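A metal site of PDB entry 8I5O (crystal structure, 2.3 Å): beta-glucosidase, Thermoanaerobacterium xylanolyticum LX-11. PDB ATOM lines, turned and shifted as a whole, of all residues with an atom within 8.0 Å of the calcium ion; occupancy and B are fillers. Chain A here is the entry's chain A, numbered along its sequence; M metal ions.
The side-chain carboxylate of Asp 564 is in hydrogen-bond range of the side-chain hydroxyl of Thr 585, 2.8 Å away. The backbone carbonyl oxygen (O) of Asp 564 lies within hydrogen-bond range of the side-chain amide nitrogen (ND2) of Asn 626 (2.7 Å). N of Lys 561 lies close to OD1 of Asp 568 (3.0 Å). The backbone carbonyl oxygen of Met 559 sits at hydrogen-bond distance from the backbone NH of Asp 568 (3.2 Å). N of Asn 563 sits close to OD1 of Asp 560 (3.2 Å). OD2 of Asp 560 sits at hydrogen-bond distance from N of Gly 565 (2.8 Å). The side-chain carboxylate (OD2) of Asp 560 is in salt-bridge range of the side-chain amino group (NZ) of Lys 557 (3.5 Å).
Five residues have an atom within 4 Å of the calcium ion: Asp 560, Asp 562, Asp 564, Ile 566 and Asp 568.
The calcium ion is bound by O of Ile 566, OD1 of Asp 564, OD1 of Asp 568, OD1 of Asp 562 and OD1 of Asp 560. The calcium ion has five donor atoms within binding distance.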
ATOM      1  N   LYS A 557      17.733 -18.859   3.675  1.00  0.00           N
ATOM      2  CA  LYS A 557      18.071 -19.680   4.845  1.00  0.00           C
ATOM      3  C   LYS A 557      17.194 -19.380   6.071  1.00  0.00           C
ATOM      4  O   LYS A 557      16.867 -20.300   6.831  1.00  0.00           O
ATOM      5  CB  LYS A 557      19.563 -19.499   5.204  1.00  0.00           C
ATOM      6  CG  LYS A 557      20.108 -20.443   6.270  1.00  0.00           C
ATOM      7  CD  LYS A 557      20.181 -21.886   5.788  1.00  0.00           C
ATOM      8  CE  LYS A 557      20.878 -22.793   6.792  1.00  0.00           C
ATOM      9  NZ  LYS A 557      19.996 -23.194   7.918  1.00  0.00           N
ATOM     10  N   MET A 559      14.070 -18.797   6.091  1.00  0.00           N
ATOM     11  CA  MET A 559      12.798 -19.502   5.913  1.00  0.00           C
ATOM     12  C   MET A 559      12.855 -20.997   6.258  1.00  0.00           C
ATOM     13  O   MET A 559      11.855 -21.702   6.107  1.00  0.00           O
ATOM     14  CB  MET A 559      12.292 -19.300   4.470  1.00  0.00           C
ATOM     15  CG  MET A 559      12.077 -17.833   4.101  1.00  0.00           C
ATOM     16  SD  MET A 559      11.603 -17.592   2.375  1.00  0.00           S
ATOM     17  CE  MET A 559      11.745 -15.818   2.242  1.00  0.00           C
ATOM     18  N   ASP A 560      14.018 -21.497   6.714  1.00  0.00           N
ATOM     19  CA  ASP A 560      14.153 -22.866   7.233  1.00  0.00           C
ATOM     20  C   ASP A 560      13.653 -22.936   8.674  1.00  0.00           C
ATOM     21  O   ASP A 560      14.390 -22.644   9.618  1.00  0.00           O
ATOM     22  CB  ASP A 560      15.616 -23.325   7.142  1.00  0.00           C
ATOM     23  CG  ASP A 560      15.835 -24.744   7.642  1.00  0.00           C
ATOM     24  OD1 ASP A 560      14.878 -25.543   7.694  1.00  0.00           O
ATOM     25  OD2 ASP A 560      16.994 -25.071   7.966  1.00  0.00           O
ATOM     26  N   LYS A 561      12.398 -23.371   8.831  1.00  0.00           N
ATOM     27  CA  LYS A 561      11.717 -23.382  10.133  1.00  0.00           C
ATOM     28  C   LYS A 561      12.118 -24.603  10.969  1.00  0.00           C
ATOM     29  O   LYS A 561      12.517 -24.452  12.126  1.00  0.00           O
ATOM     30  CB  LYS A 561      10.201 -23.374   9.932  1.00  0.00           C
ATOM     31  CG  LYS A 561       9.645 -22.205   9.117  1.00  0.00           C
ATOM     32  CD  LYS A 561       9.501 -20.907   9.909  1.00  0.00           C
ATOM     33  CE  LYS A 561      10.802 -20.125  10.019  1.00  0.00           C
ATOM     34  NZ  LYS A 561      10.568 -18.747  10.522  1.00  0.00           N
ATOM     35  N   ASP A 562      11.994 -25.788  10.382  1.00  0.00           N
ATOM     36  CA  ASP A 562      12.277 -27.050  11.104  1.00  0.00           C
ATOM     37  C   ASP A 562      13.770 -27.432  11.211  1.00  0.00           C
ATOM     38  O   ASP A 562      14.094 -28.503  11.742  1.00  0.00           O
ATOM     39  CB  ASP A 562      11.467 -28.209  10.497  1.00  0.00           C
ATOM     40  CG  ASP A 562      11.951 -28.648   9.116  1.00  0.00           C
ATOM     41  OD1 ASP A 562      12.493 -27.804   8.368  1.00  0.00           O
ATOM     42  OD2 ASP A 562      11.788 -29.833   8.776  1.00  0.00           O
ATOM     43  N   ASN A 563      14.670 -26.587  10.686  1.00  0.00           N
ATOM     44  CA  ASN A 563      16.119 -26.713  10.880  1.00  0.00           C
ATOM     45  C   ASN A 563      16.784 -27.925  10.187  1.00  0.00           C
ATOM     46  O   ASN A 563      17.753 -28.506  10.700  1.00  0.00           O
ATOM     47  CB  ASN A 563      16.457 -26.680  12.388  1.00  0.00           C
ATOM     48  CG  ASN A 563      17.848 -26.148  12.668  1.00  0.00           C
ATOM     49  OD1 ASN A 563      18.698 -26.872  13.198  1.00  0.00           O
ATOM     50  ND2 ASN A 563      18.097 -24.896  12.301  1.00  0.00           N
ATOM     51  N   ASP A 564      16.287 -28.282   8.997  1.00  0.00           N
ATOM     52  CA  ASP A 564      16.909 -29.337   8.158  1.00  0.00           C
ATOM     53  C   ASP A 564      17.892 -28.784   7.101  1.00  0.00           C
ATOM     54  O   ASP A 564      18.371 -29.539   6.259  1.00  0.00           O
ATOM     55  CB  ASP A 564      15.833 -30.239   7.503  1.00  0.00           C
ATOM     56  CG  ASP A 564      15.037 -29.532   6.388  1.00  0.00           C
ATOM     57  OD1 ASP A 564      15.054 -28.286   6.294  1.00  0.00           O
ATOM     58  OD2 ASP A 564      14.365 -30.226   5.604  1.00  0.00           O
ATOM     59  N   GLY A 565      18.176 -27.479   7.162  1.00  0.00           N
ATOM     60  CA  GLY A 565      19.096 -26.822   6.229  1.00  0.00           C
ATOM     61  C   GLY A 565      18.493 -26.410   4.890  1.00  0.00           C
ATOM     62  O   GLY A 565      19.223 -25.973   3.995  1.00  0.00           O
ATOM     63  N   ILE A 566      17.174 -26.524   4.755  1.00  0.00           N
ATOM     64  CA  ILE A 566      16.474 -26.285   3.499  1.00  0.00           C
ATOM     65  C   ILE A 566      15.295 -25.368   3.811  1.00  0.00           C
ATOM     66  O   ILE A 566      14.602 -25.597   4.791  1.00  0.00           O
ATOM     67  CB  ILE A 566      15.952 -27.618   2.906  1.00  0.00           C
ATOM     68  CG1 ILE A 566      17.103 -28.606   2.649  1.00  0.00           C
ATOM     69  CG2 ILE A 566      15.173 -27.379   1.609  1.00  0.00           C
ATOM     70  CD1 ILE A 566      16.670 -30.051   2.537  1.00  0.00           C
ATOM     71  N   PRO A 567      15.040 -24.334   2.985  1.00  0.00           N
ATOM     72  CA  PRO A 567      13.836 -23.508   3.237  1.00  0.00           C
ATOM     73  C   PRO A 567      12.542 -24.315   3.113  1.00  0.00           C
ATOM     74  O   PRO A 567      12.437 -25.160   2.237  1.00  0.00           O
ATOM     75  CB  PRO A 567      13.906 -22.427   2.152  1.00  0.00           C
ATOM     76  CG  PRO A 567      14.854 -22.940   1.124  1.00  0.00           C
ATOM     77  CD  PRO A 567      15.838 -23.785   1.866  1.00  0.00           C
ATOM     78  N   ASP A 568      11.593 -24.050   4.015  1.00  0.00           N
ATOM     79  CA  ASP A 568      10.296 -24.753   4.045  1.00  0.00           C
ATOM     80  C   ASP A 568       9.285 -24.084   3.139  1.00  0.00           C
ATOM     81  O   ASP A 568       9.022 -22.895   3.302  1.00  0.00           O
ATOM     82  CB  ASP A 568       9.687 -24.743   5.454  1.00  0.00           C
ATOM     83  CG  ASP A 568      10.419 -25.643   6.418  1.00  0.00           C
ATOM     84  OD1 ASP A 568      11.608 -25.351   6.702  1.00  0.00           O
ATOM     85  OD2 ASP A 568       9.827 -26.627   6.898  1.00  0.00           O
ATOM     86  N   ASN A 569       8.712 -24.844   2.198  1.00  0.00           N
ATOM     87  CA  ASN A 569       7.488 -24.433   1.526  1.00  0.00           C
ATOM     88  C   ASN A 569       6.352 -24.501   2.551  1.00  0.00           C
ATOM     89  O   ASN A 569       6.329 -25.402   3.382  1.00  0.00           O
ATOM     90  CB  ASN A 569       7.183 -25.301   0.303  1.00  0.00           C
ATOM     91  CG  ASN A 569       8.144 -25.084  -0.851  1.00  0.00           C
ATOM     92  OD1 ASN A 569       9.064 -25.865  -1.066  1.00  0.00           O
ATOM     93  ND2 ASN A 569       7.934 -24.005  -1.608  1.00  0.00           N
ATOM     94  N   GLY A 584       6.639 -28.171   3.186  1.00  0.00           N
ATOM     95  CA  GLY A 584       7.812 -28.822   3.762  1.00  0.00           C
ATOM     96  C   GLY A 584       9.025 -28.637   2.883  1.00  0.00           C
ATOM     97  O   GLY A 584       9.248 -27.555   2.339  1.00  0.00           O
ATOM     98  N   THR A 585       9.810 -29.697   2.736  1.00  0.00           N
ATOM     99  CA  THR A 585      10.897 -29.738   1.761  1.00  0.00           C
ATOM    100  C   THR A 585      10.305 -30.281   0.461  1.00  0.00           C
ATOM    101  O   THR A 585       9.702 -31.351   0.456  1.00  0.00           O
ATOM    102  CB  THR A 585      12.045 -30.627   2.246  1.00  0.00           C
ATOM    103  OG1 THR A 585      12.625 -30.044   3.421  1.00  0.00           O
ATOM    104  CG2 THR A 585      13.121 -30.758   1.172  1.00  0.00           C
ATOM    105  N   SER A 586      10.464 -29.525  -0.623  1.00  0.00           N
ATOM    106  CA  SER A 586       9.995 -29.942  -1.948  1.00  0.00           C
ATOM    107  C   SER A 586      11.184 -30.340  -2.809  1.00  0.00           C
ATOM    108  O   SER A 586      12.306 -29.864  -2.601  1.00  0.00           O
ATOM    109  CB  SER A 586       9.202 -28.827  -2.622  1.00  0.00           C
ATOM    110  OG  SER A 586      10.015 -27.678  -2.796  1.00  0.00           O
ATOM    111  N   TRP A 593      17.753 -24.998  -4.358  1.00  0.00           N
ATOM    112  CA  TRP A 593      18.507 -24.545  -3.179  1.00  0.00           C
ATOM    113  C   TRP A 593      19.903 -25.171  -3.118  1.00  0.00           C
ATOM    114  O   TRP A 593      20.897 -24.456  -2.945  1.00  0.00           O
ATOM    115  CB  TRP A 593      17.706 -24.851  -1.905  1.00  0.00           C
ATOM    116  CG  TRP A 593      18.411 -24.604  -0.601  1.00  0.00           C
ATOM    117  CD1 TRP A 593      18.685 -25.527   0.377  1.00  0.00           C
ATOM    118  CD2 TRP A 593      18.900 -23.353  -0.112  1.00  0.00           C
ATOM    119  NE1 TRP A 593      19.321 -24.926   1.432  1.00  0.00           N
ATOM    120  CE2 TRP A 593      19.459 -23.589   1.156  1.00  0.00           C
ATOM    121  CE3 TRP A 593      18.914 -22.050  -0.629  1.00  0.00           C
ATOM    122  CZ2 TRP A 593      20.052 -22.568   1.918  1.00  0.00           C
ATOM    123  CZ3 TRP A 593      19.493 -21.032   0.130  1.00  0.00           C
ATOM    124  CH2 TRP A 593      20.051 -21.298   1.390  1.00  0.00           C
ATOM    125  N   ASN A 626      19.982 -34.144   4.087  1.00  0.00           N
ATOM    126  CA  ASN A 626      18.562 -34.103   4.472  1.00  0.00           C
ATOM    127  C   ASN A 626      17.596 -34.191   3.286  1.00  0.00           C
ATOM    128  O   ASN A 626      16.525 -34.782   3.416  1.00  0.00           O
ATOM    129  CB  ASN A 626      18.270 -32.866   5.329  1.00  0.00           C
ATOM    130  CG  ASN A 626      18.853 -32.971   6.736  1.00  0.00           C
ATOM    131  OD1 ASN A 626      18.810 -34.031   7.350  1.00  0.00           O
ATOM    132  ND2 ASN A 626      19.385 -31.873   7.251  1.00  0.00           N
ATOM    133  N   GLU A 630      14.959 -37.260   3.138  1.00  0.00           N
ATOM    134  CA  GLU A 630      13.525 -36.912   3.171  1.00  0.00           C
ATOM    135  C   GLU A 630      12.747 -37.289   1.902  1.00  0.00           C
ATOM    136  O   GLU A 630      11.569 -37.635   1.995  1.00  0.00           O
ATOM    137  CB  GLU A 630      13.358 -35.408   3.443  1.00  0.00           C
ATOM    138  CG  GLU A 630      13.737 -34.990   4.856  1.00  0.00           C
ATOM    139  CD  GLU A 630      13.937 -33.483   4.996  1.00  0.00           C
ATOM    140  OE1 GLU A 630      13.361 -32.716   4.210  1.00  0.00           O
ATOM    141  OE2 GLU A 630      14.683 -33.081   5.911  1.00  0.00           O
ATOM    142  N   THR A 641       7.450 -33.258   1.272  1.00  0.00           N
ATOM    143  CA  THR A 641       7.356 -34.051   2.503  1.00  0.00           C
ATOM    144  C   THR A 641       6.015 -33.969   3.249  1.00  0.00           C
ATOM    145  O   THR A 641       5.721 -34.864   4.042  1.00  0.00           O
ATOM    146  CB  THR A 641       8.467 -33.669   3.508  1.00  0.00           C
ATOM    147  OG1 THR A 641       8.382 -32.271   3.827  1.00  0.00           O
ATOM    148  CG2 THR A 641       9.836 -33.969   2.929  1.00  0.00           C
ATOM    149  N   GLU A 642       5.206 -32.927   2.996  1.00  0.00           N
ATOM    150  CA  GLU A 642       4.012 -32.642   3.826  1.00  0.00           C
ATOM    151  C   GLU A 642       2.648 -32.444   3.113  1.00  0.00           C
ATOM    152  O   GLU A 642       1.638 -32.282   3.806  1.00  0.00           O
ATOM    153  CB  GLU A 642       4.298 -31.428   4.728  1.00  0.00           C
ATOM    154  CG  GLU A 642       5.350 -31.682   5.792  1.00  0.00           C
ATOM    155  CD  GLU A 642       5.692 -30.446   6.614  1.00  0.00           C
ATOM    156  OE1 GLU A 642       4.786 -29.609   6.861  1.00  0.00           O
ATOM    157  OE2 GLU A 642       6.861 -30.303   7.017  1.00  0.00           O
HETATM  158 CA    CA M   1      13.252 -26.863   6.142  1.00  0.00          CA
